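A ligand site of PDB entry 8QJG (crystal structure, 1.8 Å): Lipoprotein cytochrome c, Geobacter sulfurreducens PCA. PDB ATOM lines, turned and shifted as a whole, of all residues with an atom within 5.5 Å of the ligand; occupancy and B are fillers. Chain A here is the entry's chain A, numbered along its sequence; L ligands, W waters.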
ATOM      1  N   TYR A  30     -29.160  19.242   2.802  1.00  0.00           N
ATOM      2  CA  TYR A  30     -28.443  19.485   1.569  1.00  0.00           C
ATOM      3  C   TYR A  30     -27.669  20.801   1.648  1.00  0.00           C
ATOM      4  O   TYR A  30     -26.503  20.878   1.219  1.00  0.00           O
ATOM      5  CB  TYR A  30     -29.415  19.486   0.408  1.00  0.00           C
ATOM      6  CG  TYR A  30     -28.769  19.758  -0.905  1.00  0.00           C
ATOM      7  CD1 TYR A  30     -28.437  21.042  -1.284  1.00  0.00           C
ATOM      8  CD2 TYR A  30     -28.413  18.702  -1.754  1.00  0.00           C
ATOM      9  CE1 TYR A  30     -27.794  21.306  -2.472  1.00  0.00           C
ATOM     10  CE2 TYR A  30     -27.780  18.962  -2.997  1.00  0.00           C
ATOM     11  CZ  TYR A  30     -27.478  20.273  -3.336  1.00  0.00           C
ATOM     12  OH  TYR A  30     -26.828  20.583  -4.530  1.00  0.00           O
ATOM     13  N   ASN A  33     -24.540  20.209   3.876  1.00  0.00           N
ATOM     14  CA  ASN A  33     -23.611  19.134   3.554  1.00  0.00           C
ATOM     15  C   ASN A  33     -23.241  19.004   2.075  1.00  0.00           C
ATOM     16  O   ASN A  33     -22.231  18.358   1.778  1.00  0.00           O
ATOM     17  CB  ASN A  33     -24.177  17.771   4.029  1.00  0.00           C
ATOM     18  CG  ASN A  33     -24.268  17.681   5.545  1.00  0.00           C
ATOM     19  OD1 ASN A  33     -23.267  17.463   6.220  1.00  0.00           O
ATOM     20  ND2 ASN A  33     -25.477  17.859   6.092  1.00  0.00           N
ATOM     21  N   CYS A  34     -23.993  19.620   1.160  1.00  0.00           N
ATOM     22  CA  CYS A  34     -23.791  19.353  -0.259  1.00  0.00           C
ATOM     23  C   CYS A  34     -23.553  20.604  -1.105  1.00  0.00           C
ATOM     24  O   CYS A  34     -22.826  20.589  -2.109  1.00  0.00           O
ATOM     25  CB  CYS A  34     -24.996  18.602  -0.830  1.00  0.00           C
ATOM     26  SG  CYS A  34     -25.613  17.227   0.190  1.00  0.00           S
ATOM     27  N   CYS A  37     -20.356  22.393  -2.844  1.00  0.00           N
ATOM     28  CA  CYS A  37     -19.726  21.795  -4.023  1.00  0.00           C
ATOM     29  C   CYS A  37     -20.656  21.530  -5.193  1.00  0.00           C
ATOM     30  O   CYS A  37     -20.149  21.395  -6.307  1.00  0.00           O
ATOM     31  CB  CYS A  37     -19.093  20.439  -3.668  1.00  0.00           C
ATOM     32  SG  CYS A  37     -17.808  20.453  -2.374  1.00  0.00           S
ATOM     33  N   HIS A  38     -21.967  21.410  -4.971  1.00  0.00           N
ATOM     34  CA  HIS A  38     -22.922  20.995  -5.998  1.00  0.00           C
ATOM     35  C   HIS A  38     -23.894  22.088  -6.403  1.00  0.00           C
ATOM     36  O   HIS A  38     -24.692  21.865  -7.331  1.00  0.00           O
ATOM     37  CB  HIS A  38     -23.724  19.734  -5.543  1.00  0.00           C
ATOM     38  CG  HIS A  38     -22.956  18.466  -5.686  1.00  0.00           C
ATOM     39  ND1 HIS A  38     -22.557  17.969  -6.914  1.00  0.00           N
ATOM     40  CD2 HIS A  38     -22.530  17.564  -4.774  1.00  0.00           C
ATOM     41  CE1 HIS A  38     -21.855  16.864  -6.746  1.00  0.00           C
ATOM     42  NE2 HIS A  38     -21.854  16.568  -5.459  1.00  0.00           N
ATOM     43  N   ASP A  45     -26.112  20.354  -9.498  1.00  0.00           N
ATOM     44  CA  ASP A  45     -25.539  19.655 -10.636  1.00  0.00           C
ATOM     45  C   ASP A  45     -25.534  18.140 -10.477  1.00  0.00           C
ATOM     46  O   ASP A  45     -24.970  17.445 -11.321  1.00  0.00           O
ATOM     47  CB  ASP A  45     -24.137  20.147 -10.955  1.00  0.00           C
ATOM     48  CG  ASP A  45     -23.132  19.851  -9.852  1.00  0.00           C
ATOM     49  OD1 ASP A  45     -23.414  18.944  -9.041  1.00  0.00           O
ATOM     50  OD2 ASP A  45     -22.051  20.469  -9.876  1.00  0.00           O
ATOM     51  N   ILE A  46     -26.178  17.617  -9.440  1.00  0.00           N
ATOM     52  CA  ILE A  46     -26.210  16.182  -9.209  1.00  0.00           C
ATOM     53  C   ILE A  46     -27.120  15.504 -10.220  1.00  0.00           C
ATOM     54  O   ILE A  46     -28.259  15.932 -10.447  1.00  0.00           O
ATOM     55  CB  ILE A  46     -26.656  15.858  -7.776  1.00  0.00           C
ATOM     56  CG1 ILE A  46     -25.573  16.239  -6.774  1.00  0.00           C
ATOM     57  CG2 ILE A  46     -27.007  14.376  -7.645  1.00  0.00           C
ATOM     58  CD1 ILE A  46     -26.079  16.620  -5.399  1.00  0.00           C
ATOM     59  N   GLN A  47     -26.632  14.395 -10.788  1.00  0.00           N
ATOM     60  CA  GLN A  47     -27.425  13.651 -11.760  1.00  0.00           C
ATOM     61  C   GLN A  47     -28.344  12.623 -11.103  1.00  0.00           C
ATOM     62  O   GLN A  47     -29.547  12.594 -11.360  1.00  0.00           O
ATOM     63  CB  GLN A  47     -26.523  12.920 -12.777  1.00  0.00           C
ATOM     64  CG  GLN A  47     -27.366  12.066 -13.741  1.00  0.00           C
ATOM     65  CD  GLN A  47     -26.602  11.562 -14.953  1.00  0.00           C
ATOM     66  OE1 GLN A  47     -26.803  12.047 -16.053  1.00  0.00           O
ATOM     67  NE2 GLN A  47     -25.755  10.555 -14.763  1.00  0.00           N
ATOM     68  N   THR A  48     -27.784  11.707 -10.351  1.00  0.00           N
ATOM     69  CA  THR A  48     -28.543  10.545  -9.902  1.00  0.00           C
ATOM     70  C   THR A  48     -28.925  10.797  -8.447  1.00  0.00           C
ATOM     71  O   THR A  48     -28.111  10.668  -7.530  1.00  0.00           O
ATOM     72  CB  THR A  48     -27.781   9.238 -10.088  1.00  0.00           C
ATOM     73  OG1 THR A  48     -27.348   9.151 -11.451  1.00  0.00           O
ATOM     74  CG2 THR A  48     -28.681   8.072  -9.766  1.00  0.00           C
ATOM     75  N   ALA A  53     -27.018   6.114  -5.080  1.00  0.00           N
ATOM     76  CA  ALA A  53     -26.061   6.944  -5.800  1.00  0.00           C
ATOM     77  C   ALA A  53     -25.245   7.798  -4.842  1.00  0.00           C
ATOM     78  O   ALA A  53     -24.018   7.914  -4.967  1.00  0.00           O
ATOM     79  CB  ALA A  53     -26.783   7.824  -6.821  1.00  0.00           C
ATOM     80  N   ILE A  54     -25.908   8.389  -3.854  1.00  0.00           N
ATOM     81  CA  ILE A  54     -25.202   9.221  -2.886  1.00  0.00           C
ATOM     82  C   ILE A  54     -24.271   8.350  -2.047  1.00  0.00           C
ATOM     83  O   ILE A  54     -23.118   8.709  -1.786  1.00  0.00           O
ATOM     84  CB  ILE A  54     -26.216   9.971  -1.998  1.00  0.00           C
ATOM     85  CG1 ILE A  54     -27.084  10.889  -2.870  1.00  0.00           C
ATOM     86  CG2 ILE A  54     -25.502  10.760  -0.921  1.00  0.00           C
ATOM     87  CD1 ILE A  54     -28.335  11.407  -2.146  1.00  0.00           C
ATOM     88  N   ALA A  57     -21.195   7.439  -4.105  1.00  0.00           N
ATOM     89  CA  ALA A  57     -20.242   8.544  -4.180  1.00  0.00           C
ATOM     90  C   ALA A  57     -19.482   8.746  -2.881  1.00  0.00           C
ATOM     91  O   ALA A  57     -18.281   9.045  -2.893  1.00  0.00           O
ATOM     92  CB  ALA A  57     -20.953   9.822  -4.574  1.00  0.00           C
ATOM     93  N   ILE A  58     -20.157   8.647  -1.730  1.00  0.00           N
ATOM     94  CA  ILE A  58     -19.445   8.738  -0.462  1.00  0.00           C
ATOM     95  C   ILE A  58     -18.395   7.633  -0.377  1.00  0.00           C
ATOM     96  O   ILE A  58     -17.230   7.893  -0.061  1.00  0.00           O
ATOM     97  CB  ILE A  58     -20.427   8.706   0.734  1.00  0.00           C
ATOM     98  CG1 ILE A  58     -21.302   9.956   0.699  1.00  0.00           C
ATOM     99  CG2 ILE A  58     -19.650   8.597   2.057  1.00  0.00           C
ATOM    100  CD1 ILE A  58     -22.528   9.919   1.604  1.00  0.00           C
ATOM    101  N   ARG A  62     -15.773  10.269  -4.124  1.00  0.00           N
ATOM    102  CA  ARG A  62     -15.814  11.136  -5.266  1.00  0.00           C
ATOM    103  C   ARG A  62     -15.826  12.556  -4.733  1.00  0.00           C
ATOM    104  O   ARG A  62     -16.648  12.908  -3.867  1.00  0.00           O
ATOM    105  CB  ARG A  62     -17.039  10.886  -6.149  1.00  0.00           C
ATOM    106  CG  ARG A  62     -17.097   9.474  -6.693  1.00  0.00           C
ATOM    107  CD  ARG A  62     -18.283   9.287  -7.601  1.00  0.00           C
ATOM    108  NE  ARG A  62     -18.184  10.085  -8.822  1.00  0.00           N
ATOM    109  CZ  ARG A  62     -18.961   9.919  -9.863  1.00  0.00           C
ATOM    110  NH1 ARG A  62     -19.934   9.009  -9.850  1.00  0.00           N
ATOM    111  NH2 ARG A  62     -18.780  10.673 -10.953  1.00  0.00           N
ATOM    112  N   GLY A  63     -14.884  13.347  -5.227  1.00  0.00           N
ATOM    113  CA  GLY A  63     -14.824  14.743  -4.838  1.00  0.00           C
ATOM    114  C   GLY A  63     -14.456  14.970  -3.382  1.00  0.00           C
ATOM    115  O   GLY A  63     -14.607  16.083  -2.875  1.00  0.00           O
ATOM    116  N   GLY A  64     -13.882  13.958  -2.725  1.00  0.00           N
ATOM    117  CA  GLY A  64     -13.618  14.031  -1.308  1.00  0.00           C
ATOM    118  C   GLY A  64     -14.813  13.806  -0.396  1.00  0.00           C
ATOM    119  O   GLY A  64     -14.681  14.052   0.833  1.00  0.00           O
ATOM    120  N   MET A  65     -15.934  13.251  -0.903  1.00  0.00           N
ATOM    121  CA  MET A  65     -17.195  13.106  -0.136  1.00  0.00           C
ATOM    122  C   MET A  65     -17.099  12.045   0.970  1.00  0.00           C
ATOM    123  O   MET A  65     -18.056  11.917   1.763  1.00  0.00           O
ATOM    124  CB  MET A  65     -18.319  12.682  -1.108  1.00  0.00           C
ATOM    125  CG  MET A  65     -18.693  13.733  -2.083  1.00  0.00           C
ATOM    126  SD  MET A  65     -20.009  13.129  -3.202  1.00  0.00           S
ATOM    127  CE  MET A  65     -21.220  12.398  -1.941  1.00  0.00           C
ATOM    128  N   PHE A  67     -15.913  12.058   3.732  1.00  0.00           N
ATOM    129  CA  PHE A  67     -16.161  12.631   5.059  1.00  0.00           C
ATOM    130  C   PHE A  67     -17.648  12.576   5.433  1.00  0.00           C
ATOM    131  O   PHE A  67     -17.966  12.641   6.622  1.00  0.00           O
ATOM    132  CB  PHE A  67     -15.588  14.073   5.086  1.00  0.00           C
ATOM    133  CG  PHE A  67     -16.480  15.123   4.463  1.00  0.00           C
ATOM    134  CD1 PHE A  67     -16.422  15.416   3.096  1.00  0.00           C
ATOM    135  CD2 PHE A  67     -17.358  15.852   5.250  1.00  0.00           C
ATOM    136  CE1 PHE A  67     -17.227  16.386   2.518  1.00  0.00           C
ATOM    137  CE2 PHE A  67     -18.183  16.823   4.698  1.00  0.00           C
ATOM    138  CZ  PHE A  67     -18.133  17.082   3.304  1.00  0.00           C
ATOM    139  N   LEU A  68     -18.534  12.410   4.469  1.00  0.00           N
ATOM    140  CA  LEU A  68     -19.977  12.383   4.694  1.00  0.00           C
ATOM    141  C   LEU A  68     -20.469  11.029   5.194  1.00  0.00           C
ATOM    142  O   LEU A  68     -21.693  10.810   5.280  1.00  0.00           O
ATOM    143  CB  LEU A  68     -20.712  12.773   3.386  1.00  0.00           C
ATOM    144  CG  LEU A  68     -20.428  14.239   3.086  1.00  0.00           C
ATOM    145  CD1 LEU A  68     -20.643  14.588   1.601  1.00  0.00           C
ATOM    146  CD2 LEU A  68     -21.255  15.122   3.999  1.00  0.00           C
ATOM    147  N   LEU A  71     -23.425  10.946   7.796  1.00  0.00           N
ATOM    148  CA  LEU A  71     -24.844  11.018   7.529  1.00  0.00           C
ATOM    149  C   LEU A  71     -25.513   9.679   7.795  1.00  0.00           C
ATOM    150  O   LEU A  71     -25.010   8.622   7.405  1.00  0.00           O
ATOM    151  CB  LEU A  71     -25.113  11.453   6.091  1.00  0.00           C
ATOM    152  CG  LEU A  71     -24.808  12.902   5.646  1.00  0.00           C
ATOM    153  CD1 LEU A  71     -24.761  12.963   4.142  1.00  0.00           C
ATOM    154  CD2 LEU A  71     -25.880  13.824   6.192  1.00  0.00           C
ATOM    155  N   ILE A  79     -32.294  13.887   1.832  1.00  0.00           N
ATOM    156  CA  ILE A  79     -31.596  14.669   0.820  1.00  0.00           C
ATOM    157  C   ILE A  79     -32.011  14.226  -0.593  1.00  0.00           C
ATOM    158  O   ILE A  79     -32.308  15.063  -1.463  1.00  0.00           O
ATOM    159  CB  ILE A  79     -30.063  14.550   0.996  1.00  0.00           C
ATOM    160  CG1 ILE A  79     -29.643  15.195   2.332  1.00  0.00           C
ATOM    161  CG2 ILE A  79     -29.336  15.131  -0.210  1.00  0.00           C
ATOM    162  CD1 ILE A  79     -28.188  14.898   2.730  1.00  0.00           C
ATOM    163  N   LEU A  83     -33.856  16.465  -3.384  1.00  0.00           N
ATOM    164  CA  LEU A  83     -33.243  16.662  -4.704  1.00  0.00           C
ATOM    165  C   LEU A  83     -34.184  16.217  -5.835  1.00  0.00           C
ATOM    166  O   LEU A  83     -34.318  16.904  -6.857  1.00  0.00           O
ATOM    167  CB  LEU A  83     -31.930  15.887  -4.773  1.00  0.00           C
ATOM    168  CG  LEU A  83     -30.690  16.587  -4.264  1.00  0.00           C
ATOM    169  CD1 LEU A  83     -29.481  15.635  -4.191  1.00  0.00           C
ATOM    170  CD2 LEU A  83     -30.450  17.786  -5.149  1.00  0.00           C
HETATM  171 FE1  LIG L   1     -20.990  15.099  -4.258  1.00  0.00          FE
HETATM  172  C1  LIG L   1     -20.238  13.184  -6.971  1.00  0.00           C
HETATM  173  C2  LIG L   1     -24.136  13.683  -4.186  1.00  0.00           C
HETATM  174  C3  LIG L   1     -21.534  16.597  -1.320  1.00  0.00           C
HETATM  175  C4  LIG L   1     -18.145  16.986  -4.751  1.00  0.00           C
HETATM  176  N1  LIG L   1     -22.019  13.705  -5.324  1.00  0.00           N
HETATM  177  C5  LIG L   1     -21.506  13.053  -6.459  1.00  0.00           C
HETATM  178  C6  LIG L   1     -22.529  12.168  -6.991  1.00  0.00           C
HETATM  179  C7  LIG L   1     -23.618  12.294  -6.241  1.00  0.00           C
HETATM  180  C8  LIG L   1     -23.318  13.261  -5.204  1.00  0.00           C
HETATM  181  C9  LIG L   1     -24.968  11.558  -6.420  1.00  0.00           C
HETATM  182  C10 LIG L   1     -22.360  11.275  -8.254  1.00  0.00           C
HETATM  183  C11 LIG L   1     -22.406  12.114  -9.513  1.00  0.00           C
HETATM  184  C12 LIG L   1     -23.827  12.541  -9.878  1.00  0.00           C
HETATM  185  O1  LIG L   1     -24.017  13.723 -10.164  1.00  0.00           O
HETATM  186  O2  LIG L   1     -24.770  11.711  -9.880  1.00  0.00           O
HETATM  187  N2  LIG L   1     -22.514  15.137  -2.986  1.00  0.00           N
HETATM  188  C13 LIG L   1     -23.708  14.474  -3.156  1.00  0.00           C
HETATM  189  C14 LIG L   1     -24.502  14.726  -1.985  1.00  0.00           C
HETATM  190  C15 LIG L   1     -23.819  15.546  -1.191  1.00  0.00           C
HETATM  191  C16 LIG L   1     -22.525  15.794  -1.805  1.00  0.00           C
HETATM  192  C17 LIG L   1     -25.944  14.218  -1.830  1.00  0.00           C
HETATM  193  C18 LIG L   1     -24.243  16.109   0.159  1.00  0.00           C
HETATM  194  C19 LIG L   1     -24.603  14.937   1.097  1.00  0.00           C
HETATM  195  N3  LIG L   1     -19.999  16.587  -3.267  1.00  0.00           N
HETATM  196  C20 LIG L   1     -20.377  16.954  -1.986  1.00  0.00           C
HETATM  197  C21 LIG L   1     -19.334  17.795  -1.441  1.00  0.00           C
HETATM  198  C22 LIG L   1     -18.370  17.948  -2.383  1.00  0.00           C
HETATM  199  C23 LIG L   1     -18.781  17.164  -3.535  1.00  0.00           C
HETATM  200  C24 LIG L   1     -19.431  18.432  -0.042  1.00  0.00           C
HETATM  201  C25 LIG L   1     -17.098  18.822  -2.303  1.00  0.00           C
HETATM  202  C26 LIG L   1     -16.169  18.515  -1.112  1.00  0.00           C
HETATM  203  N4  LIG L   1     -19.438  15.065  -5.636  1.00  0.00           N
HETATM  204  C27 LIG L   1     -18.435  16.013  -5.661  1.00  0.00           C
HETATM  205  C28 LIG L   1     -17.594  15.736  -6.809  1.00  0.00           C
HETATM  206  C29 LIG L   1     -18.210  14.536  -7.506  1.00  0.00           C
HETATM  207  C30 LIG L   1     -19.384  14.204  -6.722  1.00  0.00           C
HETATM  208  C31 LIG L   1     -16.380  16.547  -7.191  1.00  0.00           C
HETATM  209  C32 LIG L   1     -17.692  13.849  -8.802  1.00  0.00           C
HETATM  210  C33 LIG L   1     -18.119  14.499 -10.089  1.00  0.00           C
HETATM  211  C34 LIG L   1     -17.195  13.899 -11.151  1.00  0.00           C
HETATM  212  O3  LIG L   1     -16.708  14.636 -12.036  1.00  0.00           O
HETATM  213  O4  LIG L   1     -16.922  12.657 -11.063  1.00  0.00           O
HETATM  214  O   HOH W   1     -24.728   9.482 -11.782  1.00  0.00           O
HETATM  215  O   HOH W   2     -15.124  10.806 -12.188  1.00  0.00           O
HETATM  216  O   HOH W   3     -17.548  17.339 -12.326  1.00  0.00           O
HETATM  217  O   HOH W   4     -13.638  13.926 -11.993  1.00  0.00           O
HETATM  218  O   HOH W   5     -15.320  11.147  -9.182  1.00  0.00           O
HETATM  219  O   HOH W   6     -22.477  15.987  -9.756  1.00  0.00           O
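A carbon (C18) of the ligand is covalently linked to the side-chain sulfur (SG) of Cys 34, 1.8 Å away.
C25 of the ligand is bonded to SG of Cys 37.
NE2 of His 38 binds FE1 of the ligand, 2.1 Å away.
The side-chain sulfur (SD) of Met 65 is bound to an iron atom (FE1) of the ligand.
An oxygen (O4) of the ligand is in salt-bridge range of the guanidinium group of Arg 62.
The backbone NH (N) of Gln 47 lies within hydrogen-bond range of an oxygen (O1) of the ligand, 2.8 Å away.
An oxygen (O2) of the ligand lies within hydrogen-bond range of the backbone NH (N) of Thr 48, at 3.1 Å.
Water W6 lies within hydrogen-bond range of O1 of the ligand, OD1 of Asp 45 and ND1 of His 38.
Water W5 lies within hydrogen-bond range of O4 of the ligand (2.9 Å) and NE of Arg 62 (3.1 Å).
Water W1 lies within hydrogen-bond range of OG1 of Thr 48 (2.7 Å), O2 of the ligand (2.9 Å) and NE2 of Gln 47 (3.3 Å).
Residues that only touch the ligand: Asn 33 (3.3 Å), Gly 63 (3.3 Å), Ile 46 (3.4 Å), Ile 54 (3.6 Å), Leu 71 (3.6 Å), Leu 68 (3.7 Å), Ala 57 (3.7 Å), Phe 67 (3.8 Å) and Ile 79 (3.9 Å).
Within 4 Å of the ligand: Asn 33, Cys 34, Cys 37, His 38, Ile 46, Gln 47, Thr 48, Ile 54, Ala 57, Arg 62, Gly 63, Met 65, Phe 67, Leu 68, Leu 71 and Ile 79.
The nearest printed residue that does not touch the ligand is Asp 45 (4.01 Å).
A ring nitrogen (ND1) of His 38 sits at hydrogen-bond distance from the side-chain carboxylate (OD1) of Asp 45 (2.5 Å).
The backbone NH of Arg 62 lies within hydrogen-bond range of the backbone carbonyl oxygen of Ala 57, at 3.1 Å.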
